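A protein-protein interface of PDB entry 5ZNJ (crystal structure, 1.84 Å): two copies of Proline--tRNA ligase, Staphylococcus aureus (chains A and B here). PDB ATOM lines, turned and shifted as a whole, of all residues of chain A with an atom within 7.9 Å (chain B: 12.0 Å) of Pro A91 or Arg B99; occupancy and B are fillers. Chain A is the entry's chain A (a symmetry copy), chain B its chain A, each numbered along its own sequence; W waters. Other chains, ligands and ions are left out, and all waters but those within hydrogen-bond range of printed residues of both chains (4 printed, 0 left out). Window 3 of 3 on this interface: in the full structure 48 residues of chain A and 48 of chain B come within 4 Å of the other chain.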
ATOM      1  N   ALA A  88     -19.452 -13.729  36.638  1.00  0.00           N
ATOM      2  CA  ALA A  88     -20.199 -12.977  37.660  1.00  0.00           C
ATOM      3  C   ALA A  88     -20.743 -11.640  37.151  1.00  0.00           C
ATOM      4  O   ALA A  88     -21.858 -11.244  37.506  1.00  0.00           O
ATOM      5  CB  ALA A  88     -19.338 -12.754  38.895  1.00  0.00           C
ATOM      6  N   TYR A  89     -19.952 -10.941  36.336  1.00  0.00           N
ATOM      7  CA  TYR A  89     -20.347  -9.623  35.823  1.00  0.00           C
ATOM      8  C   TYR A  89     -21.102  -9.726  34.506  1.00  0.00           C
ATOM      9  O   TYR A  89     -20.980 -10.715  33.774  1.00  0.00           O
ATOM     10  CB  TYR A  89     -19.125  -8.703  35.694  1.00  0.00           C
ATOM     11  CG  TYR A  89     -18.698  -8.164  37.034  1.00  0.00           C
ATOM     12  CD1 TYR A  89     -17.988  -8.962  37.934  1.00  0.00           C
ATOM     13  CD2 TYR A  89     -19.044  -6.868  37.430  1.00  0.00           C
ATOM     14  CE1 TYR A  89     -17.616  -8.476  39.178  1.00  0.00           C
ATOM     15  CE2 TYR A  89     -18.674  -6.376  38.670  1.00  0.00           C
ATOM     16  CZ  TYR A  89     -17.960  -7.185  39.538  1.00  0.00           C
ATOM     17  OH  TYR A  89     -17.592  -6.704  40.766  1.00  0.00           O
ATOM     18  N   GLY A  90     -21.883  -8.685  34.226  1.00  0.00           N
ATOM     19  CA  GLY A  90     -22.735  -8.616  33.042  1.00  0.00           C
ATOM     20  C   GLY A  90     -22.284  -7.524  32.076  1.00  0.00           C
ATOM     21  O   GLY A  90     -21.090  -7.403  31.802  1.00  0.00           O
ATOM     22  N   PRO A  91     -23.231  -6.716  31.560  1.00  0.00           N
ATOM     23  CA  PRO A  91     -22.902  -5.798  30.465  1.00  0.00           C
ATOM     24  C   PRO A  91     -21.935  -4.652  30.805  1.00  0.00           C
ATOM     25  O   PRO A  91     -21.356  -4.092  29.884  1.00  0.00           O
ATOM     26  CB  PRO A  91     -24.270  -5.239  30.051  1.00  0.00           C
ATOM     27  CG  PRO A  91     -25.102  -5.348  31.280  1.00  0.00           C
ATOM     28  CD  PRO A  91     -24.650  -6.609  31.950  1.00  0.00           C
ATOM     29  N   GLU A  92     -21.749  -4.311  32.082  1.00  0.00           N
ATOM     30  CA  GLU A  92     -20.798  -3.244  32.448  1.00  0.00           C
ATOM     31  C   GLU A  92     -19.360  -3.613  32.061  1.00  0.00           C
ATOM     32  O   GLU A  92     -18.564  -2.726  31.751  1.00  0.00           O
ATOM     33  CB  GLU A  92     -20.867  -2.878  33.936  1.00  0.00           C
ATOM     34  CG  GLU A  92     -20.109  -1.589  34.268  1.00  0.00           C
ATOM     35  CD  GLU A  92     -20.380  -1.046  35.664  1.00  0.00           C
ATOM     36  OE1 GLU A  92     -21.523  -1.153  36.151  1.00  0.00           O
ATOM     37  OE2 GLU A  92     -19.444  -0.483  36.269  1.00  0.00           O
ATOM     38  N   LEU A  93     -19.041  -4.906  32.087  1.00  0.00           N
ATOM     39  CA  LEU A  93     -17.758  -5.395  31.594  1.00  0.00           C
ATOM     40  C   LEU A  93     -17.800  -5.399  30.071  1.00  0.00           C
ATOM     41  O   LEU A  93     -18.599  -6.123  29.474  1.00  0.00           O
ATOM     42  CB  LEU A  93     -17.472  -6.804  32.134  1.00  0.00           C
ATOM     43  CG  LEU A  93     -16.116  -7.434  31.803  1.00  0.00           C
ATOM     44  CD1 LEU A  93     -14.948  -6.609  32.330  1.00  0.00           C
ATOM     45  CD2 LEU A  93     -16.053  -8.847  32.367  1.00  0.00           C
ATOM     46  N   MET A  94     -16.950  -4.583  29.443  1.00  0.00           N
ATOM     47  CA  MET A  94     -16.896  -4.520  27.985  1.00  0.00           C
ATOM     48  C   MET A  94     -16.112  -5.709  27.464  1.00  0.00           C
ATOM     49  O   MET A  94     -15.054  -6.032  27.994  1.00  0.00           O
ATOM     50  CB  MET A  94     -16.271  -3.214  27.506  1.00  0.00           C
ATOM     51  CG  MET A  94     -17.035  -1.998  27.989  1.00  0.00           C
ATOM     52  SD  MET A  94     -16.688  -0.516  27.043  1.00  0.00           S
ATOM     53  CE  MET A  94     -17.910  -0.685  25.736  1.00  0.00           C
ATOM     54  N   ARG A  95     -16.649  -6.366  26.438  1.00  0.00           N
ATOM     55  CA  ARG A  95     -16.076  -7.602  25.912  1.00  0.00           C
ATOM     56  C   ARG A  95     -15.912  -7.515  24.398  1.00  0.00           C
ATOM     57  O   ARG A  95     -16.607  -6.752  23.730  1.00  0.00           O
ATOM     58  CB  ARG A  95     -16.968  -8.792  26.270  1.00  0.00           C
ATOM     59  CG  ARG A  95     -17.200  -8.997  27.764  1.00  0.00           C
ATOM     60  CD  ARG A  95     -18.342  -9.975  28.041  1.00  0.00           C
ATOM     61  NE  ARG A  95     -18.985  -9.701  29.337  1.00  0.00           N
ATOM     62  CZ  ARG A  95     -18.893 -10.442  30.446  1.00  0.00           C
ATOM     63  NH1 ARG A  95     -18.188 -11.571  30.484  1.00  0.00           N
ATOM     64  NH2 ARG A  95     -19.529 -10.047  31.544  1.00  0.00           N
ATOM     65  N   ARG A 140     -15.685   0.881  31.499  1.00  0.00           N
ATOM     66  CA  ARG A 140     -16.885   0.353  32.159  1.00  0.00           C
ATOM     67  C   ARG A 140     -18.097   0.845  31.390  1.00  0.00           C
ATOM     68  O   ARG A 140     -18.255   2.046  31.183  1.00  0.00           O
ATOM     69  CB  ARG A 140     -16.961   0.823  33.608  1.00  0.00           C
ATOM     70  CG  ARG A 140     -15.845   0.283  34.483  1.00  0.00           C
ATOM     71  CD  ARG A 140     -15.944   0.766  35.906  1.00  0.00           C
ATOM     72  NE  ARG A 140     -14.799   0.319  36.694  1.00  0.00           N
ATOM     73  CZ  ARG A 140     -14.630   0.559  37.989  1.00  0.00           C
ATOM     74  NH1 ARG A 140     -15.542   1.246  38.683  1.00  0.00           N
ATOM     75  NH2 ARG A 140     -13.555   0.079  38.609  1.00  0.00           N
ATOM     76  N   ASP A 141     -18.940  -0.078  30.936  1.00  0.00           N
ATOM     77  CA  ASP A 141     -20.113   0.293  30.156  1.00  0.00           C
ATOM     78  C   ASP A 141     -21.224   0.676  31.132  1.00  0.00           C
ATOM     79  O   ASP A 141     -22.177  -0.087  31.370  1.00  0.00           O
ATOM     80  CB  ASP A 141     -20.523  -0.843  29.212  1.00  0.00           C
ATOM     81  CG  ASP A 141     -21.306  -0.356  28.005  1.00  0.00           C
ATOM     82  OD1 ASP A 141     -21.576   0.856  27.889  1.00  0.00           O
ATOM     83  OD2 ASP A 141     -21.647  -1.203  27.154  1.00  0.00           O
ATOM     84  N   GLU A 142     -21.069   1.870  31.701  1.00  0.00           N
ATOM     85  CA  GLU A 142     -21.933   2.364  32.774  1.00  0.00           C
ATOM     86  C   GLU A 142     -23.360   2.450  32.249  1.00  0.00           C
ATOM     87  O   GLU A 142     -23.577   2.872  31.121  1.00  0.00           O
ATOM     88  CB  GLU A 142     -21.495   3.759  33.230  1.00  0.00           C
ATOM     89  CG  GLU A 142     -20.089   3.877  33.816  1.00  0.00           C
ATOM     90  CD  GLU A 142     -19.969   3.423  35.259  1.00  0.00           C
ATOM     91  OE1 GLU A 142     -18.827   3.166  35.690  1.00  0.00           O
ATOM     92  OE2 GLU A 142     -20.988   3.330  35.975  1.00  0.00           O
ATOM     93  N   LYS A 143     -24.325   2.060  33.071  1.00  0.00           N
ATOM     94  CA  LYS A 143     -25.733   2.105  32.673  1.00  0.00           C
ATOM     95  C   LYS A 143     -26.195   3.536  32.395  1.00  0.00           C
ATOM     96  O   LYS A 143     -26.947   3.770  31.453  1.00  0.00           O
ATOM     97  CB  LYS A 143     -26.604   1.457  33.750  1.00  0.00           C
ATOM     98  CG  LYS A 143     -27.972   1.016  33.257  1.00  0.00           C
ATOM     99  CD  LYS A 143     -28.757   0.276  34.336  1.00  0.00           C
ATOM    100  CE  LYS A 143     -29.592   1.206  35.210  1.00  0.00           C
ATOM    101  NZ  LYS A 143     -28.812   2.006  36.199  1.00  0.00           N
ATOM    102  N   ARG A 144     -25.707   4.486  33.194  1.00  0.00           N
ATOM    103  CA  ARG A 144     -26.084   5.888  33.076  1.00  0.00           C
ATOM    104  C   ARG A 144     -24.868   6.818  33.217  1.00  0.00           C
ATOM    105  O   ARG A 144     -24.672   7.433  34.273  1.00  0.00           O
ATOM    106  CB  ARG A 144     -27.140   6.203  34.140  1.00  0.00           C
ATOM    107  CG  ARG A 144     -27.825   7.555  33.997  1.00  0.00           C
ATOM    108  CD  ARG A 144     -28.598   7.902  35.267  1.00  0.00           C
ATOM    109  NE  ARG A 144     -29.543   6.844  35.641  1.00  0.00           N
ATOM    110  CZ  ARG A 144     -30.175   6.746  36.813  1.00  0.00           C
ATOM    111  NH1 ARG A 144     -29.985   7.641  37.785  1.00  0.00           N
ATOM    112  NH2 ARG A 144     -31.016   5.733  37.020  1.00  0.00           N
ATOM    113  N   PRO A 145     -24.057   6.942  32.142  1.00  0.00           N
ATOM    114  CA  PRO A 145     -23.006   7.956  32.133  1.00  0.00           C
ATOM    115  C   PRO A 145     -23.633   9.331  32.336  1.00  0.00           C
ATOM    116  O   PRO A 145     -24.725   9.597  31.817  1.00  0.00           O
ATOM    117  CB  PRO A 145     -22.387   7.830  30.730  1.00  0.00           C
ATOM    118  CG  PRO A 145     -22.811   6.493  30.229  1.00  0.00           C
ATOM    119  CD  PRO A 145     -24.154   6.253  30.844  1.00  0.00           C
ATOM    120  N   ARG A 153     -17.457   6.327  30.558  1.00  0.00           N
ATOM    121  CA  ARG A 153     -17.300   4.931  30.174  1.00  0.00           C
ATOM    122  C   ARG A 153     -15.845   4.575  29.909  1.00  0.00           C
ATOM    123  O   ARG A 153     -15.444   3.437  30.121  1.00  0.00           O
ATOM    124  CB  ARG A 153     -18.163   4.618  28.957  1.00  0.00           C
ATOM    125  CG  ARG A 153     -19.643   4.713  29.284  1.00  0.00           C
ATOM    126  CD  ARG A 153     -20.483   3.993  28.252  1.00  0.00           C
ATOM    127  NE  ARG A 153     -20.600   4.755  27.011  1.00  0.00           N
ATOM    128  CZ  ARG A 153     -21.055   4.268  25.857  1.00  0.00           C
ATOM    129  NH1 ARG A 153     -21.414   2.987  25.742  1.00  0.00           N
ATOM    130  NH2 ARG A 153     -21.137   5.067  24.799  1.00  0.00           N
ATOM    131  N   LEU B  74     -11.899   4.173  22.670  1.00  0.00           N
ATOM    132  CA  LEU B  74     -13.237   3.716  22.251  1.00  0.00           C
ATOM    133  C   LEU B  74     -13.853   4.716  21.289  1.00  0.00           C
ATOM    134  O   LEU B  74     -14.168   5.839  21.680  1.00  0.00           O
ATOM    135  CB  LEU B  74     -14.177   3.557  23.449  1.00  0.00           C
ATOM    136  CG  LEU B  74     -14.224   2.225  24.174  1.00  0.00           C
ATOM    137  CD1 LEU B  74     -15.179   2.356  25.349  1.00  0.00           C
ATOM    138  CD2 LEU B  74     -14.663   1.104  23.245  1.00  0.00           C
ATOM    139  N   ARG B  95     -12.899  -4.401  16.850  1.00  0.00           N
ATOM    140  CA  ARG B  95     -14.269  -3.901  16.914  1.00  0.00           C
ATOM    141  C   ARG B  95     -15.014  -4.522  18.092  1.00  0.00           C
ATOM    142  O   ARG B  95     -14.664  -5.605  18.559  1.00  0.00           O
ATOM    143  CB  ARG B  95     -15.007  -4.213  15.611  1.00  0.00           C
ATOM    144  CG  ARG B  95     -14.367  -3.631  14.353  1.00  0.00           C
ATOM    145  CD  ARG B  95     -14.947  -4.242  13.077  1.00  0.00           C
ATOM    146  NE  ARG B  95     -13.973  -4.211  11.973  1.00  0.00           N
ATOM    147  CZ  ARG B  95     -14.018  -3.426  10.892  1.00  0.00           C
ATOM    148  NH1 ARG B  95     -15.009  -2.562  10.687  1.00  0.00           N
ATOM    149  NH2 ARG B  95     -13.047  -3.513   9.987  1.00  0.00           N
ATOM    150  N   LEU B  96     -16.028  -3.818  18.580  1.00  0.00           N
ATOM    151  CA  LEU B  96     -16.867  -4.332  19.661  1.00  0.00           C
ATOM    152  C   LEU B  96     -18.228  -3.643  19.684  1.00  0.00           C
ATOM    153  O   LEU B  96     -18.467  -2.684  18.946  1.00  0.00           O
ATOM    154  CB  LEU B  96     -16.165  -4.206  21.024  1.00  0.00           C
ATOM    155  CG  LEU B  96     -15.915  -2.817  21.628  1.00  0.00           C
ATOM    156  CD1 LEU B  96     -15.739  -2.937  23.128  1.00  0.00           C
ATOM    157  CD2 LEU B  96     -14.705  -2.130  21.006  1.00  0.00           C
ATOM    158  N   GLN B  97     -19.110  -4.170  20.524  1.00  0.00           N
ATOM    159  CA  GLN B  97     -20.443  -3.616  20.740  1.00  0.00           C
ATOM    160  C   GLN B  97     -20.618  -3.264  22.202  1.00  0.00           C
ATOM    161  O   GLN B  97     -20.191  -4.021  23.070  1.00  0.00           O
ATOM    162  CB  GLN B  97     -21.513  -4.640  20.363  1.00  0.00           C
ATOM    163  CG  GLN B  97     -21.804  -4.741  18.879  1.00  0.00           C
ATOM    164  CD  GLN B  97     -23.124  -5.448  18.611  1.00  0.00           C
ATOM    165  OE1 GLN B  97     -23.531  -6.330  19.371  1.00  0.00           O
ATOM    166  NE2 GLN B  97     -23.812  -5.052  17.541  1.00  0.00           N
ATOM    167  N   ASP B  98     -21.270  -2.135  22.477  1.00  0.00           N
ATOM    168  CA  ASP B  98     -21.650  -1.800  23.851  1.00  0.00           C
ATOM    169  C   ASP B  98     -22.982  -2.473  24.219  1.00  0.00           C
ATOM    170  O   ASP B  98     -23.573  -3.194  23.405  1.00  0.00           O
ATOM    171  CB  ASP B  98     -21.635  -0.274  24.089  1.00  0.00           C
ATOM    172  CG  ASP B  98     -22.853   0.459  23.534  1.00  0.00           C
ATOM    173  OD1 ASP B  98     -23.797  -0.162  22.984  1.00  0.00           O
ATOM    174  OD2 ASP B  98     -22.849   1.700  23.664  1.00  0.00           O
ATOM    175  N   ARG B  99     -23.437  -2.228  25.444  1.00  0.00           N
ATOM    176  CA  ARG B  99     -24.651  -2.857  25.988  1.00  0.00           C
ATOM    177  C   ARG B  99     -25.976  -2.494  25.294  1.00  0.00           C
ATOM    178  O   ARG B  99     -26.997  -3.123  25.569  1.00  0.00           O
ATOM    179  CB  ARG B  99     -24.762  -2.567  27.490  1.00  0.00           C
ATOM    180  CG  ARG B  99     -25.011  -1.105  27.849  1.00  0.00           C
ATOM    181  CD  ARG B  99     -24.764  -0.867  29.325  1.00  0.00           C
ATOM    182  NE  ARG B  99     -25.739  -1.570  30.157  1.00  0.00           N
ATOM    183  CZ  ARG B  99     -25.600  -1.848  31.454  1.00  0.00           C
ATOM    184  NH1 ARG B  99     -24.505  -1.501  32.133  1.00  0.00           N
ATOM    185  NH2 ARG B  99     -26.576  -2.491  32.089  1.00  0.00           N
ATOM    186  N   HIS B 100     -25.962  -1.472  24.436  1.00  0.00           N
ATOM    187  CA  HIS B 100     -27.114  -1.092  23.613  1.00  0.00           C
ATOM    188  C   HIS B 100     -26.963  -1.505  22.145  1.00  0.00           C
ATOM    189  O   HIS B 100     -27.740  -1.064  21.290  1.00  0.00           O
ATOM    190  CB  HIS B 100     -27.336   0.415  23.731  1.00  0.00           C
ATOM    191  CG  HIS B 100     -27.611   0.860  25.132  1.00  0.00           C
ATOM    192  ND1 HIS B 100     -26.642   1.411  25.941  1.00  0.00           N
ATOM    193  CD2 HIS B 100     -28.738   0.800  25.881  1.00  0.00           C
ATOM    194  CE1 HIS B 100     -27.164   1.689  27.122  1.00  0.00           C
ATOM    195  NE2 HIS B 100     -28.434   1.328  27.112  1.00  0.00           N
ATOM    196  N   GLY B 101     -25.981  -2.364  21.857  1.00  0.00           N
ATOM    197  CA  GLY B 101     -25.730  -2.838  20.498  1.00  0.00           C
ATOM    198  C   GLY B 101     -25.018  -1.851  19.584  1.00  0.00           C
ATOM    199  O   GLY B 101     -24.880  -2.114  18.395  1.00  0.00           O
ATOM    200  N   ARG B 102     -24.537  -0.734  20.127  1.00  0.00           N
ATOM    201  CA  ARG B 102     -23.873   0.287  19.322  1.00  0.00           C
ATOM    202  C   ARG B 102     -22.436  -0.160  19.052  1.00  0.00           C
ATOM    203  O   ARG B 102     -21.773  -0.685  19.943  1.00  0.00           O
ATOM    204  CB  ARG B 102     -23.919   1.643  20.029  1.00  0.00           C
ATOM    205  CG  ARG B 102     -25.347   2.099  20.304  1.00  0.00           C
ATOM    206  CD  ARG B 102     -25.431   3.527  20.799  1.00  0.00           C
ATOM    207  NE  ARG B 102     -26.830   3.981  20.822  1.00  0.00           N
ATOM    208  CZ  ARG B 102     -27.561   4.257  21.908  1.00  0.00           C
ATOM    209  NH1 ARG B 102     -27.065   4.161  23.146  1.00  0.00           N
ATOM    210  NH2 ARG B 102     -28.824   4.653  21.752  1.00  0.00           N
ATOM    211  N   GLN B 103     -21.976   0.045  17.821  1.00  0.00           N
ATOM    212  CA  GLN B 103     -20.706  -0.513  17.362  1.00  0.00           C
ATOM    213  C   GLN B 103     -19.564   0.480  17.537  1.00  0.00           C
ATOM    214  O   GLN B 103     -19.739   1.681  17.340  1.00  0.00           O
ATOM    215  CB  GLN B 103     -20.813  -0.947  15.901  1.00  0.00           C
ATOM    216  CG  GLN B 103     -21.779  -2.104  15.687  1.00  0.00           C
ATOM    217  CD  GLN B 103     -21.660  -2.725  14.304  1.00  0.00           C
ATOM    218  OE1 GLN B 103     -21.384  -2.032  13.321  1.00  0.00           O
ATOM    219  NE2 GLN B 103     -21.877  -4.036  14.218  1.00  0.00           N
ATOM    220  N   PHE B 104     -18.393  -0.047  17.897  1.00  0.00           N
ATOM    221  CA  PHE B 104     -17.202   0.759  18.158  1.00  0.00           C
ATOM    222  C   PHE B 104     -15.951   0.135  17.566  1.00  0.00           C
ATOM    223  O   PHE B 104     -15.872  -1.083  17.419  1.00  0.00           O
ATOM    224  CB  PHE B 104     -16.969   0.875  19.663  1.00  0.00           C
ATOM    225  CG  PHE B 104     -17.963   1.740  20.366  1.00  0.00           C
ATOM    226  CD1 PHE B 104     -19.174   1.218  20.798  1.00  0.00           C
ATOM    227  CD2 PHE B 104     -17.683   3.074  20.612  1.00  0.00           C
ATOM    228  CE1 PHE B 104     -20.095   2.016  21.455  1.00  0.00           C
ATOM    229  CE2 PHE B 104     -18.597   3.882  21.272  1.00  0.00           C
ATOM    230  CZ  PHE B 104     -19.806   3.350  21.692  1.00  0.00           C
HETATM  231  O   HOH W   1     -23.913  -0.537  34.852  1.00  0.00           O
HETATM  232  O   HOH W   2     -18.598  -6.721  21.826  1.00  0.00           O
HETATM  233  O   HOH W   3     -19.019  -4.964  25.499  1.00  0.00           O
HETATM  234  O   HOH W   4     -22.877   4.947  22.609  1.00  0.00           O
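The backbone NH (N) of Arg B99 sits at hydrogen-bond distance from the side-chain carboxylate (OD2) of Asp A141, at 2.7 Å.
The guanidinium group (NH1) of Arg A153 is in salt-bridge range of the side-chain carboxylate (OD2) of Asp B98, 2.8 Å away.
OD1 of Asp B98 lies within hydrogen-bond range of N of His B100.
The side-chain carboxylate (OD1) of Asp A141 lies within salt-bridge range of the guanidinium group (NH1) of Arg A153 (3.0 Å).
The backbone NH of Gly B101 is in hydrogen-bond range of the side-chain carboxylate of Asp B98, 3.3 Å away.
O of Arg A153 sits at hydrogen-bond distance from N of Arg A140.
O of Glu A92 sits at hydrogen-bond distance from N of Asp A141, at 2.8 Å.
The guanidinium group (NH2) of Arg A95 lies within hydrogen-bond range of the backbone carbonyl oxygen (O) of Tyr A89 (2.7 Å).
Among the printed residues, pairs that only touch across the chains: Pro A91 with Arg B99, Glu A92 with Arg B99, Met A94 with Leu B74, Arg A95 with Leu B96, Asp A141 with Asp B98, Lys A143 with Arg B99 and Arg A153 with Phe B104.
Pro A91 touches one residue of chain B.
Of chain A, only Pro A91, Glu A92, Asp A141 and Lys A143 come within 4 Å of Arg B99.
Of chain B, only Arg B99 comes within 4 Å of Glu A92.
Of chain B, only Asp B98 (3.2 Å) and Arg B99 (2.7 Å) come within 4 Å of Asp A141.
Of chain B, only Arg B99 comes within 4 Å of Lys A143.
Of the printed residues of chain B, Met A94 touches Leu B74.
Of the printed residues of chain B, Arg A95 touches Leu B96.
The nearest residue of chain B that does not touch Pro A91 is Asp B98 (6.1 Å).
The nearest printed residue of chain A that does not touch Phe B104 is Met A94 (5.4 Å).
Of the 15 printed residues of chain A, 7 touch a printed residue of chain B.
Hydrophobic or aromatic side chains of chain A within 4 Å of the printed part of chain B: Pro A91 and Met A94.
Of the 11 printed residues of chain B, 5 touch a printed residue of chain A.
Position printed for both chains: 95.
Of the 9 pairs that touch across the chains among the printed residues, none has its exchanged pair printed and touching as well.
Water W2 bridges the backbone carbonyl oxygen of Arg A95 and the backbone NH of Gln B97.
Water W1 lies within hydrogen-bond range of OE1 of Glu A92 (2.8 Å), NH1 of Arg B99 (2.9 Å) and N of Lys A143 (3.2 Å).
Water W4 lies within hydrogen-bond range of the guanidinium group of Arg A153 (2.8 Å) and the side-chain carboxylate of Asp B98 (3.4 Å).
Water W3 lies within hydrogen-bond range of the backbone carbonyl oxygen (O) of Gln B97 (2.9 Å) and the backbone NH (N) of Arg A95 (2.9 Å).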
